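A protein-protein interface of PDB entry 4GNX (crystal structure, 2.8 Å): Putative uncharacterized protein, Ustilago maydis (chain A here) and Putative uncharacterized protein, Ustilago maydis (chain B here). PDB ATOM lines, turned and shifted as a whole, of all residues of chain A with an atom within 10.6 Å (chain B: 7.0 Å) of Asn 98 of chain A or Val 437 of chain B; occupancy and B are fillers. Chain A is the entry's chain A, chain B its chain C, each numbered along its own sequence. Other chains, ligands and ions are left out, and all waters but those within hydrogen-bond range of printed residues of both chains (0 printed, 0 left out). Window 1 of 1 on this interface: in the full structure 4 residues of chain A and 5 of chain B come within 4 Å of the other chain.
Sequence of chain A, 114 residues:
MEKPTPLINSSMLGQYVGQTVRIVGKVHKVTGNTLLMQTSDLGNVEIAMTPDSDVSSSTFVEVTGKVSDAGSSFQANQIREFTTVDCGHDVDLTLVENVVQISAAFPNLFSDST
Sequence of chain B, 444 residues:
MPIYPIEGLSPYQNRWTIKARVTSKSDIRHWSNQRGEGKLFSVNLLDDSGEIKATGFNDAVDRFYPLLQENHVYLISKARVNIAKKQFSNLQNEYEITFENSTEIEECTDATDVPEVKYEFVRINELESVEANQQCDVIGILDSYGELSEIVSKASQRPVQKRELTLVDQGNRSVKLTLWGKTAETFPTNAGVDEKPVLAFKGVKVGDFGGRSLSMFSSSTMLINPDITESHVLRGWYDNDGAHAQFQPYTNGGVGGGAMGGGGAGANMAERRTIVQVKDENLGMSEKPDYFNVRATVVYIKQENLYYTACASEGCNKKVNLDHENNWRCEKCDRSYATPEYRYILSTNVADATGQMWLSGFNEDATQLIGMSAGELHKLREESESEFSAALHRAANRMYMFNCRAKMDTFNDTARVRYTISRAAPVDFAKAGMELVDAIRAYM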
ATOM      1  N   LEU A   7     -27.620 -22.917 -19.501  1.00  0.00           N
ATOM      2  CA  LEU A   7     -27.119 -24.285 -19.706  1.00  0.00           C
ATOM      3  C   LEU A   7     -25.947 -24.153 -20.608  1.00  0.00           C
ATOM      4  O   LEU A   7     -26.103 -23.745 -21.759  1.00  0.00           O
ATOM      5  CB  LEU A   7     -28.162 -25.141 -20.418  1.00  0.00           C
ATOM      6  CG  LEU A   7     -28.002 -26.651 -20.364  1.00  0.00           C
ATOM      7  CD1 LEU A   7     -28.072 -27.174 -18.930  1.00  0.00           C
ATOM      8  CD2 LEU A   7     -29.059 -27.299 -21.240  1.00  0.00           C
ATOM      9  N   ILE A   8     -24.763 -24.483 -20.120  1.00  0.00           N
ATOM     10  CA  ILE A   8     -23.584 -24.206 -20.920  1.00  0.00           C
ATOM     11  C   ILE A   8     -22.681 -25.427 -21.100  1.00  0.00           C
ATOM     12  O   ILE A   8     -22.856 -26.447 -20.430  1.00  0.00           O
ATOM     13  CB  ILE A   8     -22.815 -22.956 -20.388  1.00  0.00           C
ATOM     14  CG1 ILE A   8     -22.047 -23.287 -19.116  1.00  0.00           C
ATOM     15  CG2 ILE A   8     -23.765 -21.777 -20.182  1.00  0.00           C
ATOM     16  CD1 ILE A   8     -20.742 -22.545 -19.015  1.00  0.00           C
ATOM     17  N   ASN A   9     -21.764 -25.328 -22.054  1.00  0.00           N
ATOM     18  CA  ASN A   9     -20.709 -26.291 -22.197  1.00  0.00           C
ATOM     19  C   ASN A   9     -19.398 -25.625 -21.776  1.00  0.00           C
ATOM     20  O   ASN A   9     -19.408 -24.472 -21.330  1.00  0.00           O
ATOM     21  CB  ASN A   9     -20.679 -26.866 -23.621  1.00  0.00           C
ATOM     22  CG  ASN A   9     -20.532 -25.801 -24.715  1.00  0.00           C
ATOM     23  OD1 ASN A   9     -21.124 -25.940 -25.783  1.00  0.00           O
ATOM     24  ND2 ASN A   9     -19.708 -24.775 -24.481  1.00  0.00           N
ATOM     25  N   MET A  12     -18.150 -22.094 -23.118  1.00  0.00           N
ATOM     26  CA  MET A  12     -18.872 -20.896 -22.734  1.00  0.00           C
ATOM     27  C   MET A  12     -18.462 -20.362 -21.366  1.00  0.00           C
ATOM     28  O   MET A  12     -18.901 -19.298 -20.955  1.00  0.00           O
ATOM     29  CB  MET A  12     -20.371 -21.149 -22.781  1.00  0.00           C
ATOM     30  CG  MET A  12     -20.861 -21.411 -24.194  1.00  0.00           C
ATOM     31  SD  MET A  12     -22.539 -22.064 -24.349  1.00  0.00           S
ATOM     32  CE  MET A  12     -23.541 -20.705 -23.736  1.00  0.00           C
ATOM     33  N   VAL A  24     -23.822 -30.026 -17.660  1.00  0.00           N
ATOM     34  CA  VAL A  24     -24.011 -31.474 -17.621  1.00  0.00           C
ATOM     35  C   VAL A  24     -22.800 -32.200 -18.177  1.00  0.00           C
ATOM     36  O   VAL A  24     -22.234 -31.807 -19.190  1.00  0.00           O
ATOM     37  CB  VAL A  24     -25.233 -31.924 -18.453  1.00  0.00           C
ATOM     38  CG1 VAL A  24     -25.455 -33.425 -18.303  1.00  0.00           C
ATOM     39  CG2 VAL A  24     -26.498 -31.193 -18.023  1.00  0.00           C
ATOM     40  N   THR A  39     -17.889 -32.602 -20.907  1.00  0.00           N
ATOM     41  CA  THR A  39     -19.059 -31.886 -21.394  1.00  0.00           C
ATOM     42  C   THR A  39     -19.469 -32.325 -22.800  1.00  0.00           C
ATOM     43  O   THR A  39     -18.659 -32.898 -23.517  1.00  0.00           O
ATOM     44  CB  THR A  39     -18.811 -30.371 -21.439  1.00  0.00           C
ATOM     45  OG1 THR A  39     -18.006 -29.987 -20.341  1.00  0.00           O
ATOM     46  CG2 THR A  39     -20.105 -29.667 -21.257  1.00  0.00           C
ATOM     47  N   SER A  40     -20.724 -32.040 -23.177  1.00  0.00           N
ATOM     48  CA  SER A  40     -21.219 -32.198 -24.546  1.00  0.00           C
ATOM     49  C   SER A  40     -20.276 -31.560 -25.544  1.00  0.00           C
ATOM     50  O   SER A  40     -20.150 -32.001 -26.679  1.00  0.00           O
ATOM     51  CB  SER A  40     -22.591 -31.545 -24.675  1.00  0.00           C
ATOM     52  OG  SER A  40     -22.547 -30.170 -24.331  1.00  0.00           O
ATOM     53  N   ASP A  41     -19.638 -30.496 -25.085  1.00  0.00           N
ATOM     54  CA  ASP A  41     -18.587 -29.777 -25.766  1.00  0.00           C
ATOM     55  C   ASP A  41     -17.413 -30.666 -26.158  1.00  0.00           C
ATOM     56  O   ASP A  41     -16.631 -30.313 -27.040  1.00  0.00           O
ATOM     57  CB  ASP A  41     -18.068 -28.743 -24.772  1.00  0.00           C
ATOM     58  CG  ASP A  41     -17.588 -27.487 -25.438  1.00  0.00           C
ATOM     59  OD1 ASP A  41     -16.540 -26.966 -25.019  1.00  0.00           O
ATOM     60  OD2 ASP A  41     -18.249 -27.012 -26.378  1.00  0.00           O
ATOM     61  N   LEU A  42     -17.294 -31.808 -25.483  1.00  0.00           N
ATOM     62  CA  LEU A  42     -16.106 -32.681 -25.490  1.00  0.00           C
ATOM     63  C   LEU A  42     -14.950 -32.161 -24.667  1.00  0.00           C
ATOM     64  O   LEU A  42     -13.909 -32.806 -24.582  1.00  0.00           O
ATOM     65  CB  LEU A  42     -15.628 -33.033 -26.891  1.00  0.00           C
ATOM     66  CG  LEU A  42     -16.458 -34.108 -27.588  1.00  0.00           C
ATOM     67  CD1 LEU A  42     -15.714 -34.604 -28.817  1.00  0.00           C
ATOM     68  CD2 LEU A  42     -16.803 -35.258 -26.650  1.00  0.00           C
ATOM     69  N   ASP A  92     -27.821 -38.668 -23.302  1.00  0.00           N
ATOM     70  CA  ASP A  92     -27.322 -38.522 -24.671  1.00  0.00           C
ATOM     71  C   ASP A  92     -26.646 -37.182 -24.854  1.00  0.00           C
ATOM     72  O   ASP A  92     -27.312 -36.174 -25.095  1.00  0.00           O
ATOM     73  CB  ASP A  92     -28.457 -38.633 -25.691  1.00  0.00           C
ATOM     74  CG  ASP A  92     -27.965 -38.473 -27.145  1.00  0.00           C
ATOM     75  OD1 ASP A  92     -26.835 -37.946 -27.330  1.00  0.00           O
ATOM     76  OD2 ASP A  92     -28.701 -38.873 -28.096  1.00  0.00           O
ATOM     77  N   LEU A  93     -25.320 -37.187 -24.802  1.00  0.00           N
ATOM     78  CA  LEU A  93     -24.516 -35.962 -24.861  1.00  0.00           C
ATOM     79  C   LEU A  93     -24.636 -35.136 -26.145  1.00  0.00           C
ATOM     80  O   LEU A  93     -24.601 -33.910 -26.077  1.00  0.00           O
ATOM     81  CB  LEU A  93     -23.050 -36.271 -24.547  1.00  0.00           C
ATOM     82  CG  LEU A  93     -22.507 -35.753 -23.208  1.00  0.00           C
ATOM     83  CD1 LEU A  93     -23.561 -35.610 -22.112  1.00  0.00           C
ATOM     84  CD2 LEU A  93     -21.350 -36.610 -22.717  1.00  0.00           C
ATOM     85  N   THR A  94     -24.791 -35.798 -27.290  1.00  0.00           N
ATOM     86  CA  THR A  94     -25.019 -35.106 -28.544  1.00  0.00           C
ATOM     87  C   THR A  94     -26.342 -34.346 -28.491  1.00  0.00           C
ATOM     88  O   THR A  94     -26.427 -33.187 -28.922  1.00  0.00           O
ATOM     89  CB  THR A  94     -25.037 -36.081 -29.729  1.00  0.00           C
ATOM     90  OG1 THR A  94     -23.819 -36.823 -29.758  1.00  0.00           O
ATOM     91  CG2 THR A  94     -25.176 -35.339 -31.032  1.00  0.00           C
ATOM     92  N   LEU A  95     -27.377 -34.986 -27.951  1.00  0.00           N
ATOM     93  CA  LEU A  95     -28.628 -34.284 -27.748  1.00  0.00           C
ATOM     94  C   LEU A  95     -28.346 -33.046 -26.933  1.00  0.00           C
ATOM     95  O   LEU A  95     -28.814 -31.956 -27.274  1.00  0.00           O
ATOM     96  CB  LEU A  95     -29.659 -35.156 -27.029  1.00  0.00           C
ATOM     97  CG  LEU A  95     -31.015 -34.494 -26.716  1.00  0.00           C
ATOM     98  CD1 LEU A  95     -31.432 -33.491 -27.783  1.00  0.00           C
ATOM     99  CD2 LEU A  95     -32.075 -35.574 -26.557  1.00  0.00           C
ATOM    100  N   VAL A  96     -27.565 -33.213 -25.871  1.00  0.00           N
ATOM    101  CA  VAL A  96     -27.308 -32.119 -24.962  1.00  0.00           C
ATOM    102  C   VAL A  96     -26.608 -30.956 -25.671  1.00  0.00           C
ATOM    103  O   VAL A  96     -26.946 -29.783 -25.421  1.00  0.00           O
ATOM    104  CB  VAL A  96     -26.500 -32.570 -23.727  1.00  0.00           C
ATOM    105  CG1 VAL A  96     -26.094 -31.359 -22.893  1.00  0.00           C
ATOM    106  CG2 VAL A  96     -27.325 -33.541 -22.890  1.00  0.00           C
ATOM    107  N   GLU A  97     -25.664 -31.273 -26.560  1.00  0.00           N
ATOM    108  CA  GLU A  97     -24.886 -30.226 -27.182  1.00  0.00           C
ATOM    109  C   GLU A  97     -25.826 -29.325 -27.957  1.00  0.00           C
ATOM    110  O   GLU A  97     -25.739 -28.088 -27.891  1.00  0.00           O
ATOM    111  CB  GLU A  97     -23.786 -30.798 -28.064  1.00  0.00           C
ATOM    112  CG  GLU A  97     -22.924 -29.756 -28.783  1.00  0.00           C
ATOM    113  CD  GLU A  97     -22.331 -28.671 -27.874  1.00  0.00           C
ATOM    114  OE1 GLU A  97     -22.015 -28.958 -26.690  1.00  0.00           O
ATOM    115  OE2 GLU A  97     -22.169 -27.515 -28.354  1.00  0.00           O
ATOM    116  N   ASN A  98     -26.773 -29.966 -28.631  1.00  0.00           N
ATOM    117  CA  ASN A  98     -27.713 -29.288 -29.475  1.00  0.00           C
ATOM    118  C   ASN A  98     -28.677 -28.413 -28.712  1.00  0.00           C
ATOM    119  O   ASN A  98     -29.039 -27.314 -29.152  1.00  0.00           O
ATOM    120  CB  ASN A  98     -28.452 -30.315 -30.289  1.00  0.00           C
ATOM    121  CG  ASN A  98     -27.662 -30.745 -31.502  1.00  0.00           C
ATOM    122  OD1 ASN A  98     -27.490 -29.970 -32.442  1.00  0.00           O
ATOM    123  ND2 ASN A  98     -27.169 -31.977 -31.490  1.00  0.00           N
ATOM    124  N   VAL A  99     -29.094 -28.898 -27.557  1.00  0.00           N
ATOM    125  CA  VAL A  99     -29.973 -28.137 -26.724  1.00  0.00           C
ATOM    126  C   VAL A  99     -29.230 -26.920 -26.201  1.00  0.00           C
ATOM    127  O   VAL A  99     -29.794 -25.832 -26.133  1.00  0.00           O
ATOM    128  CB  VAL A  99     -30.485 -29.018 -25.602  1.00  0.00           C
ATOM    129  CG1 VAL A  99     -31.270 -28.207 -24.568  1.00  0.00           C
ATOM    130  CG2 VAL A  99     -31.333 -30.109 -26.227  1.00  0.00           C
ATOM    131  N   VAL A 100     -27.948 -27.083 -25.878  1.00  0.00           N
ATOM    132  CA  VAL A 100     -27.161 -25.933 -25.432  1.00  0.00           C
ATOM    133  C   VAL A 100     -27.163 -24.859 -26.512  1.00  0.00           C
ATOM    134  O   VAL A 100     -27.594 -23.726 -26.266  1.00  0.00           O
ATOM    135  CB  VAL A 100     -25.725 -26.294 -25.074  1.00  0.00           C
ATOM    136  CG1 VAL A 100     -24.857 -25.032 -25.041  1.00  0.00           C
ATOM    137  CG2 VAL A 100     -25.714 -26.998 -23.739  1.00  0.00           C
ATOM    138  N   GLN A 101     -26.717 -25.235 -27.703  1.00  0.00           N
ATOM    139  CA  GLN A 101     -26.649 -24.324 -28.799  1.00  0.00           C
ATOM    140  C   GLN A 101     -27.996 -23.661 -29.075  1.00  0.00           C
ATOM    141  O   GLN A 101     -28.059 -22.435 -29.255  1.00  0.00           O
ATOM    142  CB  GLN A 101     -26.172 -25.070 -30.023  1.00  0.00           C
ATOM    143  CG  GLN A 101     -24.678 -25.279 -30.118  1.00  0.00           C
ATOM    144  CD  GLN A 101     -24.294 -25.663 -31.544  1.00  0.00           C
ATOM    145  OE1 GLN A 101     -24.262 -26.856 -31.890  1.00  0.00           O
ATOM    146  NE2 GLN A 101     -24.046 -24.651 -32.402  1.00  0.00           N
ATOM    147  N   ILE A 102     -29.070 -24.461 -29.106  1.00  0.00           N
ATOM    148  CA  ILE A 102     -30.410 -23.961 -29.466  1.00  0.00           C
ATOM    149  C   ILE A 102     -30.937 -23.019 -28.395  1.00  0.00           C
ATOM    150  O   ILE A 102     -31.531 -21.977 -28.705  1.00  0.00           O
ATOM    151  CB  ILE A 102     -31.422 -25.101 -29.686  1.00  0.00           C
ATOM    152  CG1 ILE A 102     -31.126 -25.828 -30.991  1.00  0.00           C
ATOM    153  CG2 ILE A 102     -32.819 -24.554 -29.828  1.00  0.00           C
ATOM    154  CD1 ILE A 102     -31.778 -27.193 -31.131  1.00  0.00           C
ATOM    155  N   SER A 103     -30.715 -23.393 -27.135  1.00  0.00           N
ATOM    156  CA  SER A 103     -31.113 -22.547 -26.012  1.00  0.00           C
ATOM    157  C   SER A 103     -30.401 -21.201 -26.056  1.00  0.00           C
ATOM    158  O   SER A 103     -31.012 -20.178 -25.743  1.00  0.00           O
ATOM    159  CB  SER A 103     -30.869 -23.224 -24.662  1.00  0.00           C
ATOM    160  OG  SER A 103     -31.476 -24.514 -24.583  1.00  0.00           O
ATOM    161  N   ALA A 104     -29.133 -21.185 -26.459  1.00  0.00           N
ATOM    162  CA  ALA A 104     -28.420 -19.931 -26.619  1.00  0.00           C
ATOM    163  C   ALA A 104     -29.084 -19.058 -27.690  1.00  0.00           C
ATOM    164  O   ALA A 104     -29.050 -17.831 -27.604  1.00  0.00           O
ATOM    165  CB  ALA A 104     -26.957 -20.197 -26.933  1.00  0.00           C
ATOM    166  N   ALA A 105     -29.718 -19.688 -28.681  1.00  0.00           N
ATOM    167  CA  ALA A 105     -30.319 -18.956 -29.790  1.00  0.00           C
ATOM    168  C   ALA A 105     -31.728 -18.499 -29.530  1.00  0.00           C
ATOM    169  O   ALA A 105     -32.341 -17.944 -30.416  1.00  0.00           O
ATOM    170  CB  ALA A 105     -30.298 -19.802 -31.040  1.00  0.00           C
ATOM    171  N   PHE A 106     -32.280 -18.772 -28.348  1.00  0.00           N
ATOM    172  CA  PHE A 106     -33.673 -18.351 -28.036  1.00  0.00           C
ATOM    173  C   PHE A 106     -33.795 -17.678 -26.679  1.00  0.00           C
ATOM    174  O   PHE A 106     -34.530 -18.152 -25.820  1.00  0.00           O
ATOM    175  CB  PHE A 106     -34.655 -19.514 -28.147  1.00  0.00           C
ATOM    176  CG  PHE A 106     -34.865 -19.990 -29.555  1.00  0.00           C
ATOM    177  CD1 PHE A 106     -34.015 -20.937 -30.127  1.00  0.00           C
ATOM    178  CD2 PHE A 106     -35.902 -19.486 -30.320  1.00  0.00           C
ATOM    179  CE1 PHE A 106     -34.210 -21.377 -31.436  1.00  0.00           C
ATOM    180  CE2 PHE A 106     -36.106 -19.920 -31.624  1.00  0.00           C
ATOM    181  CZ  PHE A 106     -35.269 -20.874 -32.181  1.00  0.00           C
ATOM    182  N   PHE A 110     -35.241 -18.723 -22.787  1.00  0.00           N
ATOM    183  CA  PHE A 110     -34.326 -19.257 -21.773  1.00  0.00           C
ATOM    184  C   PHE A 110     -33.609 -18.204 -20.920  1.00  0.00           C
ATOM    185  O   PHE A 110     -32.832 -18.531 -20.020  1.00  0.00           O
ATOM    186  CB  PHE A 110     -33.351 -20.207 -22.427  1.00  0.00           C
ATOM    187  CG  PHE A 110     -34.021 -21.346 -23.160  1.00  0.00           C
ATOM    188  CD1 PHE A 110     -34.099 -21.345 -24.556  1.00  0.00           C
ATOM    189  CD2 PHE A 110     -34.597 -22.422 -22.460  1.00  0.00           C
ATOM    190  CE1 PHE A 110     -34.720 -22.392 -25.237  1.00  0.00           C
ATOM    191  CE2 PHE A 110     -35.224 -23.458 -23.147  1.00  0.00           C
ATOM    192  CZ  PHE A 110     -35.282 -23.448 -24.529  1.00  0.00           C
ATOM    193  N   ALA B 430     -34.519 -39.411 -26.094  1.00  0.00           N
ATOM    194  CA  ALA B 430     -33.301 -39.156 -26.855  1.00  0.00           C
ATOM    195  C   ALA B 430     -33.563 -38.979 -28.352  1.00  0.00           C
ATOM    196  O   ALA B 430     -33.143 -37.997 -28.974  1.00  0.00           O
ATOM    197  CB  ALA B 430     -32.325 -40.289 -26.640  1.00  0.00           C
ATOM    198  N   LYS B 431     -34.279 -39.947 -28.907  1.00  0.00           N
ATOM    199  CA  LYS B 431     -34.566 -39.999 -30.316  1.00  0.00           C
ATOM    200  C   LYS B 431     -35.669 -38.973 -30.725  1.00  0.00           C
ATOM    201  O   LYS B 431     -35.512 -38.241 -31.721  1.00  0.00           O
ATOM    202  CB  LYS B 431     -34.886 -41.459 -30.673  1.00  0.00           C
ATOM    203  CG  LYS B 431     -35.484 -41.659 -32.040  1.00  0.00           C
ATOM    204  CD  LYS B 431     -35.919 -43.090 -32.329  1.00  0.00           C
ATOM    205  CE  LYS B 431     -37.440 -43.206 -32.525  1.00  0.00           C
ATOM    206  NZ  LYS B 431     -38.201 -41.912 -32.678  1.00  0.00           N
ATOM    207  N   ALA B 432     -36.766 -38.891 -29.971  1.00  0.00           N
ATOM    208  CA  ALA B 432     -37.730 -37.787 -30.181  1.00  0.00           C
ATOM    209  C   ALA B 432     -37.010 -36.427 -30.127  1.00  0.00           C
ATOM    210  O   ALA B 432     -37.345 -35.500 -30.868  1.00  0.00           O
ATOM    211  CB  ALA B 432     -38.843 -37.829 -29.160  1.00  0.00           C
ATOM    212  N   GLY B 433     -36.003 -36.334 -29.259  1.00  0.00           N
ATOM    213  CA  GLY B 433     -35.152 -35.163 -29.171  1.00  0.00           C
ATOM    214  C   GLY B 433     -34.427 -34.811 -30.452  1.00  0.00           C
ATOM    215  O   GLY B 433     -34.513 -33.675 -30.923  1.00  0.00           O
ATOM    216  N   MET B 434     -33.711 -35.766 -31.031  1.00  0.00           N
ATOM    217  CA  MET B 434     -32.963 -35.485 -32.255  1.00  0.00           C
ATOM    218  C   MET B 434     -33.886 -35.090 -33.401  1.00  0.00           C
ATOM    219  O   MET B 434     -33.540 -34.222 -34.203  1.00  0.00           O
ATOM    220  CB  MET B 434     -32.055 -36.652 -32.641  1.00  0.00           C
ATOM    221  CG  MET B 434     -30.873 -36.853 -31.702  1.00  0.00           C
ATOM    222  SD  MET B 434     -29.876 -35.363 -31.396  1.00  0.00           S
ATOM    223  CE  MET B 434     -29.353 -34.880 -33.040  1.00  0.00           C
ATOM    224  N   GLU B 435     -35.066 -35.707 -33.452  1.00  0.00           N
ATOM    225  CA  GLU B 435     -36.094 -35.301 -34.407  1.00  0.00           C
ATOM    226  C   GLU B 435     -36.373 -33.828 -34.275  1.00  0.00           C
ATOM    227  O   GLU B 435     -36.256 -33.085 -35.229  1.00  0.00           O
ATOM    228  CB  GLU B 435     -37.386 -36.089 -34.209  1.00  0.00           C
ATOM    229  CG  GLU B 435     -37.471 -37.310 -35.108  1.00  0.00           C
ATOM    230  CD  GLU B 435     -38.273 -38.469 -34.506  1.00  0.00           C
ATOM    231  OE1 GLU B 435     -39.238 -38.188 -33.736  1.00  0.00           O
ATOM    232  OE2 GLU B 435     -37.947 -39.657 -34.816  1.00  0.00           O
ATOM    233  N   LEU B 436     -36.716 -33.414 -33.072  1.00  0.00           N
ATOM    234  CA  LEU B 436     -36.942 -32.010 -32.788  1.00  0.00           C
ATOM    235  C   LEU B 436     -35.767 -31.095 -33.142  1.00  0.00           C
ATOM    236  O   LEU B 436     -35.990 -29.982 -33.626  1.00  0.00           O
ATOM    237  CB  LEU B 436     -37.328 -31.803 -31.320  1.00  0.00           C
ATOM    238  CG  LEU B 436     -38.782 -32.094 -30.931  1.00  0.00           C
ATOM    239  CD1 LEU B 436     -39.017 -32.134 -29.422  1.00  0.00           C
ATOM    240  CD2 LEU B 436     -39.615 -31.017 -31.573  1.00  0.00           C
ATOM    241  N   VAL B 437     -34.531 -31.550 -32.901  1.00  0.00           N
ATOM    242  CA  VAL B 437     -33.369 -30.775 -33.333  1.00  0.00           C
ATOM    243  C   VAL B 437     -33.460 -30.491 -34.817  1.00  0.00           C
ATOM    244  O   VAL B 437     -33.437 -29.329 -35.226  1.00  0.00           O
ATOM    245  CB  VAL B 437     -32.044 -31.449 -33.022  1.00  0.00           C
ATOM    246  CG1 VAL B 437     -30.900 -30.547 -33.419  1.00  0.00           C
ATOM    247  CG2 VAL B 437     -31.949 -31.710 -31.536  1.00  0.00           C
ATOM    248  N   ASP B 438     -33.615 -31.547 -35.610  1.00  0.00           N
ATOM    249  CA  ASP B 438     -33.744 -31.399 -37.049  1.00  0.00           C
ATOM    250  C   ASP B 438     -34.835 -30.406 -37.342  1.00  0.00           C
ATOM    251  O   ASP B 438     -34.651 -29.504 -38.132  1.00  0.00           O
ATOM    252  CB  ASP B 438     -34.117 -32.726 -37.710  1.00  0.00           C
ATOM    253  CG  ASP B 438     -32.969 -33.724 -37.747  1.00  0.00           C
ATOM    254  OD1 ASP B 438     -31.787 -33.330 -37.587  1.00  0.00           O
ATOM    255  OD2 ASP B 438     -33.261 -34.929 -37.949  1.00  0.00           O
ATOM    256  N   ALA B 439     -35.974 -30.566 -36.686  1.00  0.00           N
ATOM    257  CA  ALA B 439     -37.134 -29.754 -37.001  1.00  0.00           C
ATOM    258  C   ALA B 439     -36.811 -28.281 -36.761  1.00  0.00           C
ATOM    259  O   ALA B 439     -37.054 -27.444 -37.609  1.00  0.00           O
ATOM    260  CB  ALA B 439     -38.335 -30.209 -36.185  1.00  0.00           C
ATOM    261  N   ILE B 440     -36.220 -27.995 -35.606  1.00  0.00           N
ATOM    262  CA  ILE B 440     -35.810 -26.640 -35.211  1.00  0.00           C
ATOM    263  C   ILE B 440     -34.745 -25.982 -36.120  1.00  0.00           C
ATOM    264  O   ILE B 440     -34.910 -24.826 -36.556  1.00  0.00           O
ATOM    265  CB  ILE B 440     -35.372 -26.612 -33.729  1.00  0.00           C
ATOM    266  CG1 ILE B 440     -36.544 -27.008 -32.822  1.00  0.00           C
ATOM    267  CG2 ILE B 440     -34.858 -25.240 -33.353  1.00  0.00           C
ATOM    268  CD1 ILE B 440     -36.174 -27.353 -31.403  1.00  0.00           C
ATOM    269  N   ARG B 441     -33.670 -26.712 -36.411  1.00  0.00           N
ATOM    270  CA  ARG B 441     -32.611 -26.185 -37.279  1.00  0.00           C
ATOM    271  C   ARG B 441     -33.154 -25.653 -38.608  1.00  0.00           C
ATOM    272  O   ARG B 441     -32.538 -24.782 -39.227  1.00  0.00           O
ATOM    273  CB  ARG B 441     -31.543 -27.238 -37.556  1.00  0.00           C
ATOM    274  CG  ARG B 441     -30.766 -27.681 -36.334  1.00  0.00           C
ATOM    275  CD  ARG B 441     -29.618 -26.743 -36.035  1.00  0.00           C
ATOM    276  NE  ARG B 441     -28.789 -27.213 -34.921  1.00  0.00           N
ATOM    277  CZ  ARG B 441     -27.941 -26.444 -34.238  1.00  0.00           C
ATOM    278  NH1 ARG B 441     -27.807 -25.156 -34.568  1.00  0.00           N
ATOM    279  NH2 ARG B 441     -27.237 -26.960 -33.226  1.00  0.00           N
ATOM    280  N   ALA B 442     -34.305 -26.176 -39.037  1.00  0.00           N
ATOM    281  CA  ALA B 442     -34.980 -25.711 -40.258  1.00  0.00           C
ATOM    282  C   ALA B 442     -35.571 -24.291 -40.140  1.00  0.00           C
ATOM    283  O   ALA B 442     -35.794 -23.642 -41.158  1.00  0.00           O
ATOM    284  CB  ALA B 442     -36.038 -26.699 -40.698  1.00  0.00           C
ATOM    285  N   MET B 444     -33.785 -22.147 -38.273  1.00  0.00           N
ATOM    286  CA  MET B 444     -32.550 -21.378 -38.062  1.00  0.00           C
ATOM    287  C   MET B 444     -31.523 -21.664 -39.157  1.00  0.00           C
ATOM    288  O   MET B 444     -31.267 -20.842 -40.024  1.00  0.00           O
ATOM    289  CB  MET B 444     -31.907 -21.754 -36.743  1.00  0.00           C
ATOM    290  CG  MET B 444     -32.831 -21.852 -35.551  1.00  0.00           C
ATOM    291  SD  MET B 444     -32.046 -22.902 -34.298  1.00  0.00           S
ATOM    292  CE  MET B 444     -30.337 -22.340 -34.335  1.00  0.00           C
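OD1 of Asn 98 of chain A lies within hydrogen-bond range of NH2 of Arg 441 of chain B (3.1 Å). The side-chain amide oxygen (OE1) of Gln 101 of chain A is in hydrogen-bond range of the guanidinium group (NH2) of Arg 441 of chain B.
Among the printed residues, pairs that only touch across the chains: Leu 95 of chain A with Ala 430 of chain B (3.6 Å), Asn 98 of chain A with Val 437 of chain B (3.6 Å), Phe 106 of chain A with Met 444 of chain B (3.9 Å) and Asn 98 of chain A with Met 434 of chain B (3.9 Å).
Of chain B, only Met 434, Val 437 and Arg 441 come within 4 Å of Asn 98 of chain A. Of chain A, only Asn 98 (3.6 Å) comes within 4 Å of Val 437 of chain B. Gly 433 of chain B touches none of the printed residues of chain A. No residue of chain A comes within 4 Å of Leu 436 of chain B. No residue of chain A comes within 4 Å of Asp 438 of chain B. No residue of chain A comes within 4 Å of Ala 439 of chain B. No residue of chain A comes within 4 Å of Ile 440 of chain B. Printed residues of chain A within 4 Å of Met 434 of chain B: Asn 98. Of the printed residues of chain A, Ala 430 of chain B touches Leu 95 (3.6 Å). Printed residues of chain B within 4 Å of Gln 101 of chain A: Arg 441 (3.3 Å). Printed residues of chain B within 4 Å of Phe 106 of chain A: Met 444 (3.9 Å). Val 24 of chain A touches none of the printed residues of chain B. Lys 431 of chain B touches none of the printed residues of chain A. The nearest printed residue of chain B that does not touch Asn 98 of chain A is Gly 433 of chain B (7.0 Å). The nearest residue of chain A that does not touch Val 437 of chain B is Ile 102 of chain A (4.2 Å).
Of the 14 printed residues of chain B, 5 touch a printed residue of chain A. Hydrophobic or aromatic side chains of chain B within 4 Å of the printed part of chain A: Met 434, Val 437 and Met 444. Of the 25 printed residues of chain A, 4 touch a printed residue of chain B. Printed residues of chain A that touch a printed residue of chain B: Leu 95, Asn 98, Gln 101 and Phe 106. Hydrophobic or aromatic side chains of chain A within 4 Å of the printed part of chain B: Leu 95 and Phe 106. Among the printed residues, 6 pairs touch across the chains. Among the printed residues, no Asp or Glu carboxylate lies within 4 Å of a Lys or Arg side-chain nitrogen of the other chain.
OD1 of Asp 92 of chain A is in hydrogen-bond range of N of Leu 95 of chain A (3.1 Å). The backbone carbonyl oxygen (O) of Thr 94 of chain A lies within hydrogen-bond range of the side-chain amide nitrogen (ND2) of Asn 98 of chain A (2.9 Å).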
